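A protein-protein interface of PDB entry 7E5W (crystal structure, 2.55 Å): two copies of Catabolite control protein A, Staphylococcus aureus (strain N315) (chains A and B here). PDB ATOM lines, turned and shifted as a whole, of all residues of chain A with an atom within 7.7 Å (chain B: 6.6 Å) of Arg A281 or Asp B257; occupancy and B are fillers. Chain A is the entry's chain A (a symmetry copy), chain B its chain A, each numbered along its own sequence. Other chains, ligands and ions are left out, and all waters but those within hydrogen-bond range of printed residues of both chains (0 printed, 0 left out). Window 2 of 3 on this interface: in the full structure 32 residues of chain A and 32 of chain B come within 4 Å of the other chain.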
ATOM      1  N   ILE A 249     -32.775 -14.486   6.438  1.00  0.00           N
ATOM      2  CA  ILE A 249     -31.391 -14.557   5.894  1.00  0.00           C
ATOM      3  C   ILE A 249     -30.607 -15.570   6.733  1.00  0.00           C
ATOM      4  O   ILE A 249     -29.823 -16.329   6.148  1.00  0.00           O
ATOM      5  CB  ILE A 249     -30.762 -13.152   5.786  1.00  0.00           C
ATOM      6  CG1 ILE A 249     -31.322 -12.394   4.582  1.00  0.00           C
ATOM      7  CG2 ILE A 249     -29.244 -13.202   5.748  1.00  0.00           C
ATOM      8  CD1 ILE A 249     -31.291 -10.896   4.737  1.00  0.00           C
ATOM      9  N   MET A 252     -31.683 -18.943   5.523  1.00  0.00           N
ATOM     10  CA  MET A 252     -31.140 -19.188   4.164  1.00  0.00           C
ATOM     11  C   MET A 252     -29.676 -19.616   4.252  1.00  0.00           C
ATOM     12  O   MET A 252     -29.348 -20.678   3.719  1.00  0.00           O
ATOM     13  CB  MET A 252     -31.258 -17.934   3.297  1.00  0.00           C
ATOM     14  CG  MET A 252     -31.033 -18.175   1.823  1.00  0.00           C
ATOM     15  SD  MET A 252     -30.822 -16.628   0.917  1.00  0.00           S
ATOM     16  CE  MET A 252     -29.823 -15.690   2.070  1.00  0.00           C
ATOM     17  N   HIS A 253     -28.839 -18.817   4.908  1.00  0.00           N
ATOM     18  CA  HIS A 253     -27.389 -19.123   4.972  1.00  0.00           C
ATOM     19  C   HIS A 253     -27.154 -20.427   5.736  1.00  0.00           C
ATOM     20  O   HIS A 253     -26.399 -21.247   5.230  1.00  0.00           O
ATOM     21  CB  HIS A 253     -26.613 -17.934   5.540  1.00  0.00           C
ATOM     22  CG  HIS A 253     -26.443 -16.809   4.579  1.00  0.00           C
ATOM     23  ND1 HIS A 253     -26.064 -17.010   3.270  1.00  0.00           N
ATOM     24  CD2 HIS A 253     -26.594 -15.478   4.730  1.00  0.00           C
ATOM     25  CE1 HIS A 253     -25.991 -15.849   2.654  1.00  0.00           C
ATOM     26  NE2 HIS A 253     -26.311 -14.894   3.528  1.00  0.00           N
ATOM     27  N   MET A 256     -28.000 -23.239   3.341  1.00  0.00           N
ATOM     28  CA  MET A 256     -27.088 -23.382   2.231  1.00  0.00           C
ATOM     29  C   MET A 256     -25.740 -23.865   2.707  1.00  0.00           C
ATOM     30  O   MET A 256     -25.085 -24.630   2.011  1.00  0.00           O
ATOM     31  CB  MET A 256     -26.961 -22.078   1.458  1.00  0.00           C
ATOM     32  CG  MET A 256     -28.225 -21.684   0.719  1.00  0.00           C
ATOM     33  SD  MET A 256     -27.966 -20.277  -0.367  1.00  0.00           S
ATOM     34  CE  MET A 256     -27.204 -19.126   0.760  1.00  0.00           C
ATOM     35  N   VAL A 262     -31.354 -23.775  -2.180  1.00  0.00           N
ATOM     36  CA  VAL A 262     -32.382 -22.779  -2.087  1.00  0.00           C
ATOM     37  C   VAL A 262     -32.394 -22.057  -3.443  1.00  0.00           C
ATOM     38  O   VAL A 262     -31.331 -21.556  -3.824  1.00  0.00           O
ATOM     39  CB  VAL A 262     -32.096 -21.776  -0.961  1.00  0.00           C
ATOM     40  CG1 VAL A 262     -33.080 -20.620  -0.985  1.00  0.00           C
ATOM     41  CG2 VAL A 262     -32.121 -22.468   0.390  1.00  0.00           C
ATOM     42  N   LEU A 276     -32.103  -4.999   3.318  1.00  0.00           N
ATOM     43  CA  LEU A 276     -31.279  -6.241   3.369  1.00  0.00           C
ATOM     44  C   LEU A 276     -31.712  -7.226   2.289  1.00  0.00           C
ATOM     45  O   LEU A 276     -30.913  -8.108   1.954  1.00  0.00           O
ATOM     46  CB  LEU A 276     -31.436  -6.870   4.756  1.00  0.00           C
ATOM     47  CG  LEU A 276     -30.226  -6.788   5.679  1.00  0.00           C
ATOM     48  CD1 LEU A 276     -30.457  -7.641   6.911  1.00  0.00           C
ATOM     49  CD2 LEU A 276     -28.967  -7.241   4.961  1.00  0.00           C
ATOM     50  N   VAL A 277     -32.919  -7.067   1.754  1.00  0.00           N
ATOM     51  CA  VAL A 277     -33.472  -8.024   0.752  1.00  0.00           C
ATOM     52  C   VAL A 277     -32.559  -8.078  -0.475  1.00  0.00           C
ATOM     53  O   VAL A 277     -32.394  -9.176  -1.030  1.00  0.00           O
ATOM     54  CB  VAL A 277     -34.926  -7.640   0.410  1.00  0.00           C
ATOM     55  CG1 VAL A 277     -35.345  -7.996  -1.007  1.00  0.00           C
ATOM     56  CG2 VAL A 277     -35.911  -8.193   1.425  1.00  0.00           C
ATOM     57  N   GLU A 278     -31.936  -6.957  -0.839  1.00  0.00           N
ATOM     58  CA  GLU A 278     -31.110  -6.909  -2.073  1.00  0.00           C
ATOM     59  C   GLU A 278     -29.626  -7.088  -1.743  1.00  0.00           C
ATOM     60  O   GLU A 278     -28.852  -7.362  -2.670  1.00  0.00           O
ATOM     61  CB  GLU A 278     -31.357  -5.587  -2.799  1.00  0.00           C
ATOM     62  CG  GLU A 278     -30.709  -4.398  -2.116  1.00  0.00           C
ATOM     63  CD  GLU A 278     -31.108  -3.044  -2.668  1.00  0.00           C
ATOM     64  OE1 GLU A 278     -31.338  -2.950  -3.886  1.00  0.00           O
ATOM     65  OE2 GLU A 278     -31.182  -2.088  -1.874  1.00  0.00           O
ATOM     66  N   MET A 279     -29.256  -6.974  -0.473  1.00  0.00           N
ATOM     67  CA  MET A 279     -27.830  -7.054  -0.078  1.00  0.00           C
ATOM     68  C   MET A 279     -27.385  -8.510   0.036  1.00  0.00           C
ATOM     69  O   MET A 279     -26.247  -8.728   0.454  1.00  0.00           O
ATOM     70  CB  MET A 279     -27.621  -6.377   1.278  1.00  0.00           C
ATOM     71  CG  MET A 279     -28.068  -4.936   1.324  1.00  0.00           C
ATOM     72  SD  MET A 279     -27.813  -4.238   2.970  1.00  0.00           S
ATOM     73  CE  MET A 279     -27.972  -2.490   2.614  1.00  0.00           C
ATOM     74  N   VAL A 280     -28.239  -9.464  -0.328  1.00  0.00           N
ATOM     75  CA  VAL A 280     -27.881 -10.891  -0.112  1.00  0.00           C
ATOM     76  C   VAL A 280     -28.033 -11.663  -1.412  1.00  0.00           C
ATOM     77  O   VAL A 280     -28.748 -11.181  -2.287  1.00  0.00           O
ATOM     78  CB  VAL A 280     -28.714 -11.538   1.009  1.00  0.00           C
ATOM     79  CG1 VAL A 280     -28.249 -11.101   2.387  1.00  0.00           C
ATOM     80  CG2 VAL A 280     -30.204 -11.303   0.828  1.00  0.00           C
ATOM     81  N   ARG A 281     -27.329 -12.786  -1.525  1.00  0.00           N
ATOM     82  CA  ARG A 281     -27.434 -13.661  -2.714  1.00  0.00           C
ATOM     83  C   ARG A 281     -27.578 -15.094  -2.200  1.00  0.00           C
ATOM     84  O   ARG A 281     -26.688 -15.527  -1.465  1.00  0.00           O
ATOM     85  CB  ARG A 281     -26.197 -13.535  -3.608  1.00  0.00           C
ATOM     86  CG  ARG A 281     -25.622 -12.136  -3.750  1.00  0.00           C
ATOM     87  CD  ARG A 281     -26.293 -11.325  -4.840  1.00  0.00           C
ATOM     88  NE  ARG A 281     -26.038  -9.909  -4.635  1.00  0.00           N
ATOM     89  CZ  ARG A 281     -26.670  -8.932  -5.265  1.00  0.00           C
ATOM     90  NH1 ARG A 281     -27.605  -9.219  -6.155  1.00  0.00           N
ATOM     91  NH2 ARG A 281     -26.364  -7.674  -5.012  1.00  0.00           N
ATOM     92  N   PRO A 282     -28.605 -15.921  -2.605  1.00  0.00           N
ATOM     93  CA  PRO A 282     -29.882 -15.530  -3.280  1.00  0.00           C
ATOM     94  C   PRO A 282     -30.621 -14.311  -2.713  1.00  0.00           C
ATOM     95  O   PRO A 282     -30.632 -14.140  -1.522  1.00  0.00           O
ATOM     96  CB  PRO A 282     -30.775 -16.760  -3.168  1.00  0.00           C
ATOM     97  CG  PRO A 282     -29.815 -17.886  -3.312  1.00  0.00           C
ATOM     98  CD  PRO A 282     -28.620 -17.404  -2.521  1.00  0.00           C
ATOM     99  N   GLN A 283     -31.185 -13.487  -3.594  1.00  0.00           N
ATOM    100  CA  GLN A 283     -31.967 -12.309  -3.140  1.00  0.00           C
ATOM    101  C   GLN A 283     -33.237 -12.807  -2.455  1.00  0.00           C
ATOM    102  O   GLN A 283     -33.737 -13.869  -2.832  1.00  0.00           O
ATOM    103  CB  GLN A 283     -32.168 -11.297  -4.266  1.00  0.00           C
ATOM    104  CG  GLN A 283     -31.117 -10.201  -4.292  1.00  0.00           C
ATOM    105  CD  GLN A 283     -31.320  -9.228  -5.427  1.00  0.00           C
ATOM    106  OE1 GLN A 283     -30.643  -8.210  -5.521  1.00  0.00           O
ATOM    107  NE2 GLN A 283     -32.259  -9.543  -6.302  1.00  0.00           N
ATOM    108  N   LEU A 284     -33.743 -12.056  -1.491  1.00  0.00           N
ATOM    109  CA  LEU A 284     -34.862 -12.576  -0.676  1.00  0.00           C
ATOM    110  C   LEU A 284     -36.231 -12.279  -1.277  1.00  0.00           C
ATOM    111  O   LEU A 284     -36.524 -11.110  -1.522  1.00  0.00           O
ATOM    112  CB  LEU A 284     -34.725 -11.988   0.730  1.00  0.00           C
ATOM    113  CG  LEU A 284     -35.520 -12.649   1.850  1.00  0.00           C
ATOM    114  CD1 LEU A 284     -35.390 -14.159   1.814  1.00  0.00           C
ATOM    115  CD2 LEU A 284     -35.047 -12.124   3.188  1.00  0.00           C
ATOM    116  N   GLY A 326     -35.748 -15.235  -5.914  1.00  0.00           N
ATOM    117  CA  GLY A 326     -34.523 -16.011  -5.601  1.00  0.00           C
ATOM    118  C   GLY A 326     -34.607 -17.016  -4.475  1.00  0.00           C
ATOM    119  O   GLY A 326     -33.914 -18.029  -4.560  1.00  0.00           O
ATOM    120  N   THR A 327     -35.379 -16.732  -3.433  1.00  0.00           N
ATOM    121  CA  THR A 327     -35.573 -17.738  -2.362  1.00  0.00           C
ATOM    122  C   THR A 327     -36.846 -18.517  -2.667  1.00  0.00           C
ATOM    123  O   THR A 327     -37.131 -19.462  -1.941  1.00  0.00           O
ATOM    124  CB  THR A 327     -35.472 -17.101  -0.976  1.00  0.00           C
ATOM    125  OG1 THR A 327     -36.395 -16.018  -0.911  1.00  0.00           O
ATOM    126  CG2 THR A 327     -34.074 -16.611  -0.676  1.00  0.00           C
ATOM    127  N   TYR B 222     -25.748   0.620   1.418  1.00  0.00           N
ATOM    128  CA  TYR B 222     -25.342  -0.367   0.392  1.00  0.00           C
ATOM    129  C   TYR B 222     -25.407   0.307  -0.976  1.00  0.00           C
ATOM    130  O   TYR B 222     -24.544   0.034  -1.804  1.00  0.00           O
ATOM    131  CB  TYR B 222     -26.270  -1.579   0.507  1.00  0.00           C
ATOM    132  CG  TYR B 222     -26.276  -2.559  -0.640  1.00  0.00           C
ATOM    133  CD1 TYR B 222     -27.121  -2.395  -1.726  1.00  0.00           C
ATOM    134  CD2 TYR B 222     -25.478  -3.688  -0.612  1.00  0.00           C
ATOM    135  CE1 TYR B 222     -27.132  -3.296  -2.775  1.00  0.00           C
ATOM    136  CE2 TYR B 222     -25.475  -4.598  -1.653  1.00  0.00           C
ATOM    137  CZ  TYR B 222     -26.305  -4.402  -2.739  1.00  0.00           C
ATOM    138  OH  TYR B 222     -26.315  -5.300  -3.766  1.00  0.00           O
ATOM    139  N   PHE B 229     -18.805   1.877  -6.348  1.00  0.00           N
ATOM    140  CA  PHE B 229     -18.197   0.976  -7.315  1.00  0.00           C
ATOM    141  C   PHE B 229     -18.349   1.500  -8.735  1.00  0.00           C
ATOM    142  O   PHE B 229     -17.434   1.355  -9.553  1.00  0.00           O
ATOM    143  CB  PHE B 229     -18.786  -0.421  -7.225  1.00  0.00           C
ATOM    144  CG  PHE B 229     -18.166  -1.369  -8.200  1.00  0.00           C
ATOM    145  CD1 PHE B 229     -16.850  -1.798  -8.020  1.00  0.00           C
ATOM    146  CD2 PHE B 229     -18.873  -1.820  -9.311  1.00  0.00           C
ATOM    147  CE1 PHE B 229     -16.242  -2.676  -8.932  1.00  0.00           C
ATOM    148  CE2 PHE B 229     -18.290  -2.707 -10.215  1.00  0.00           C
ATOM    149  CZ  PHE B 229     -16.965  -3.131 -10.027  1.00  0.00           C
ATOM    150  N   LYS B 233     -15.309   1.707 -11.268  1.00  0.00           N
ATOM    151  CA  LYS B 233     -15.316   0.552 -12.164  1.00  0.00           C
ATOM    152  C   LYS B 233     -14.201   0.631 -13.209  1.00  0.00           C
ATOM    153  O   LYS B 233     -13.670  -0.402 -13.636  1.00  0.00           O
ATOM    154  CB  LYS B 233     -16.693   0.448 -12.834  1.00  0.00           C
ATOM    155  CG  LYS B 233     -16.906  -0.781 -13.701  1.00  0.00           C
ATOM    156  CD  LYS B 233     -18.349  -0.821 -14.193  1.00  0.00           C
ATOM    157  CE  LYS B 233     -18.620  -2.029 -15.077  1.00  0.00           C
ATOM    158  NZ  LYS B 233     -18.661  -3.265 -14.274  1.00  0.00           N
ATOM    159  N   ILE B 249     -20.363  -3.753   1.685  1.00  0.00           N
ATOM    160  CA  ILE B 249     -21.141  -4.881   1.103  1.00  0.00           C
ATOM    161  C   ILE B 249     -21.631  -4.449  -0.282  1.00  0.00           C
ATOM    162  O   ILE B 249     -21.610  -5.286  -1.195  1.00  0.00           O
ATOM    163  CB  ILE B 249     -22.236  -5.364   2.078  1.00  0.00           C
ATOM    164  CG1 ILE B 249     -21.634  -6.205   3.203  1.00  0.00           C
ATOM    165  CG2 ILE B 249     -23.352  -6.111   1.367  1.00  0.00           C
ATOM    166  CD1 ILE B 249     -22.435  -6.180   4.479  1.00  0.00           C
ATOM    167  N   MET B 252     -18.681  -4.789  -2.557  1.00  0.00           N
ATOM    168  CA  MET B 252     -18.375  -6.224  -2.776  1.00  0.00           C
ATOM    169  C   MET B 252     -19.326  -6.812  -3.817  1.00  0.00           C
ATOM    170  O   MET B 252     -18.837  -7.367  -4.803  1.00  0.00           O
ATOM    171  CB  MET B 252     -18.493  -7.010  -1.469  1.00  0.00           C
ATOM    172  CG  MET B 252     -17.896  -8.397  -1.524  1.00  0.00           C
ATOM    173  SD  MET B 252     -18.386  -9.392  -0.099  1.00  0.00           S
ATOM    174  CE  MET B 252     -20.102  -8.911   0.080  1.00  0.00           C
ATOM    175  N   HIS B 253     -20.632  -6.682  -3.602  1.00  0.00           N
ATOM    176  CA  HIS B 253     -21.619  -7.291  -4.525  1.00  0.00           C
ATOM    177  C   HIS B 253     -21.521  -6.648  -5.909  1.00  0.00           C
ATOM    178  O   HIS B 253     -21.483  -7.397  -6.876  1.00  0.00           O
ATOM    179  CB  HIS B 253     -23.025  -7.236  -3.924  1.00  0.00           C
ATOM    180  CG  HIS B 253     -23.259  -8.232  -2.843  1.00  0.00           C
ATOM    181  ND1 HIS B 253     -22.872  -9.549  -2.959  1.00  0.00           N
ATOM    182  CD2 HIS B 253     -23.841  -8.113  -1.632  1.00  0.00           C
ATOM    183  CE1 HIS B 253     -23.202 -10.199  -1.863  1.00  0.00           C
ATOM    184  NE2 HIS B 253     -23.798  -9.340  -1.035  1.00  0.00           N
ATOM    185  N   SER B 254     -21.453  -5.320  -5.993  1.00  0.00           N
ATOM    186  CA  SER B 254     -21.296  -4.675  -7.295  1.00  0.00           C
ATOM    187  C   SER B 254     -20.095  -5.238  -8.058  1.00  0.00           C
ATOM    188  O   SER B 254     -20.196  -5.548  -9.252  1.00  0.00           O
ATOM    189  CB  SER B 254     -21.167  -3.159  -7.115  1.00  0.00           C
ATOM    190  OG  SER B 254     -22.269  -2.624  -6.384  1.00  0.00           O
ATOM    191  N   ALA B 255     -18.946  -5.381  -7.388  1.00  0.00           N
ATOM    192  CA  ALA B 255     -17.752  -5.889  -8.068  1.00  0.00           C
ATOM    193  C   ALA B 255     -17.905  -7.358  -8.448  1.00  0.00           C
ATOM    194  O   ALA B 255     -17.521  -7.763  -9.552  1.00  0.00           O
ATOM    195  CB  ALA B 255     -16.518  -5.703  -7.189  1.00  0.00           C
ATOM    196  N   MET B 256     -18.484  -8.172  -7.586  1.00  0.00           N
ATOM    197  CA  MET B 256     -18.618  -9.570  -7.922  1.00  0.00           C
ATOM    198  C   MET B 256     -19.627  -9.758  -9.028  1.00  0.00           C
ATOM    199  O   MET B 256     -19.455 -10.631  -9.870  1.00  0.00           O
ATOM    200  CB  MET B 256     -18.988 -10.393  -6.697  1.00  0.00           C
ATOM    201  CG  MET B 256     -17.884 -10.470  -5.661  1.00  0.00           C
ATOM    202  SD  MET B 256     -18.264 -11.637  -4.350  1.00  0.00           S
ATOM    203  CE  MET B 256     -19.889 -11.080  -3.873  1.00  0.00           C
ATOM    204  N   ASP B 257     -20.684  -8.961  -9.039  1.00  0.00           N
ATOM    205  CA  ASP B 257     -21.616  -8.996 -10.166  1.00  0.00           C
ATOM    206  C   ASP B 257     -20.931  -8.599 -11.466  1.00  0.00           C
ATOM    207  O   ASP B 257     -21.222  -9.162 -12.522  1.00  0.00           O
ATOM    208  CB  ASP B 257     -22.807  -8.084  -9.899  1.00  0.00           C
ATOM    209  CG  ASP B 257     -23.673  -8.579  -8.761  1.00  0.00           C
ATOM    210  OD1 ASP B 257     -23.491  -9.733  -8.306  1.00  0.00           O
ATOM    211  OD2 ASP B 257     -24.539  -7.803  -8.309  1.00  0.00           O
ATOM    212  N   ALA B 258     -20.009  -7.647 -11.415  1.00  0.00           N
ATOM    213  CA  ALA B 258     -19.257  -7.286 -12.606  1.00  0.00           C
ATOM    214  C   ALA B 258     -18.104  -8.249 -12.895  1.00  0.00           C
ATOM    215  O   ALA B 258     -17.225  -7.929 -13.704  1.00  0.00           O
ATOM    216  CB  ALA B 258     -18.725  -5.857 -12.475  1.00  0.00           C
ATOM    217  N   GLY B 259     -18.055  -9.405 -12.237  1.00  0.00           N
ATOM    218  CA  GLY B 259     -17.042 -10.397 -12.519  1.00  0.00           C
ATOM    219  C   GLY B 259     -15.759 -10.308 -11.705  1.00  0.00           C
ATOM    220  O   GLY B 259     -14.996 -11.278 -11.700  1.00  0.00           O
ATOM    221  N   ILE B 260     -15.493  -9.186 -11.018  1.00  0.00           N
ATOM    222  CA  ILE B 260     -14.235  -9.029 -10.284  1.00  0.00           C
ATOM    223  C   ILE B 260     -14.158 -10.032  -9.140  1.00  0.00           C
ATOM    224  O   ILE B 260     -15.136 -10.256  -8.412  1.00  0.00           O
ATOM    225  CB  ILE B 260     -14.087  -7.594  -9.750  1.00  0.00           C
ATOM    226  CG1 ILE B 260     -14.546  -6.583 -10.796  1.00  0.00           C
ATOM    227  CG2 ILE B 260     -12.642  -7.313  -9.370  1.00  0.00           C
ATOM    228  CD1 ILE B 260     -13.471  -6.223 -11.765  1.00  0.00           C
ATOM    229  N   ARG B 281     -21.777 -13.436   2.153  1.00  0.00           N
ATOM    230  CA  ARG B 281     -20.756 -14.374   1.639  1.00  0.00           C
ATOM    231  C   ARG B 281     -20.196 -13.763   0.353  1.00  0.00           C
ATOM    232  O   ARG B 281     -20.996 -13.510  -0.551  1.00  0.00           O
ATOM    233  CB  ARG B 281     -21.360 -15.753   1.357  1.00  0.00           C
ATOM    234  CG  ARG B 281     -22.396 -16.240   2.356  1.00  0.00           C
ATOM    235  CD  ARG B 281     -21.785 -16.932   3.557  1.00  0.00           C
ATOM    236  NE  ARG B 281     -22.740 -16.963   4.652  1.00  0.00           N
ATOM    237  CZ  ARG B 281     -22.440 -17.281   5.901  1.00  0.00           C
ATOM    238  NH1 ARG B 281     -21.199 -17.602   6.220  1.00  0.00           N
ATOM    239  NH2 ARG B 281     -23.380 -17.283   6.827  1.00  0.00           N
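Among the printed residues, merely in contact across the chains: His A253 with Arg B281 (3.5 Å), Met A279 with Tyr B222 (2.9 Å) and Arg A281 with His B253 (3.5 Å).
Printed residues of chain A that touch a printed residue of chain B: His A253, Glu A278, Met A279 and Arg A281. Hydrophobic or aromatic side chains of chain A that line the printed part of chain B: His A253 and Met A279. Printed residues of chain B that touch a printed residue of chain A: Tyr B222, His B253, Asp B257 and Arg B281. Hydrophobic or aromatic side chains of chain B within 4 Å of the printed part of chain A: Tyr B222 and His B253. Along chain B the printed residues that touch a printed residue of chain A span positions 222 to 281.
A ring nitrogen (NE2) of His B253 is in hydrogen-bond range of the backbone carbonyl oxygen of Met A279 (2.9 Å). OH of Tyr B222 sits at hydrogen-bond distance from O of Glu A278 (3.4 Å). OD2 of Asp B257 is in salt-bridge range of NH2 of Arg A281 (3.8 Å). OH of Tyr B222 lies within hydrogen-bond range of NH2 of Arg A281 (2.7 Å).
OE1 of Gln A283 lies close to O of Glu A278. The side-chain amide oxygen (OE1) of Gln A283 is in hydrogen-bond range of the guanidinium group (NH1) of Arg A281 (3.3 Å). The backbone carbonyl oxygen (O) of Glu A278 lies within hydrogen-bond range of the guanidinium group (NH2) of Arg A281 (3.4 Å).
Arg A281 touches just these residues of chain B: Tyr B222, His B253 and Asp B257. Asp B257 touches just one residue of chain A: Arg A281 (3.8 Å). Printed residues of chain A within 4 Å of Tyr B222: Glu A278 (3.4 Å), Met A279 (2.9 Å) and Arg A281 (2.7 Å). Printed residues of chain A within 4 Å of His B253: Met A279 and Arg A281. Of the printed residues of chain A, Arg B281 touches His A253 (3.5 Å). The nearest residue of chain A that does not touch Asp B257 is Gln A283 (6.7 Å). The nearest printed residue of chain A that does not touch His B253 is Val A280 (4.5 Å).
His A253 touches Arg B281, and with the chains exchanged Arg A281 touches His B253. Of the 7 pairs that touch across the chains among the printed residues, 2 have their exchanged pair printed and touching as well.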
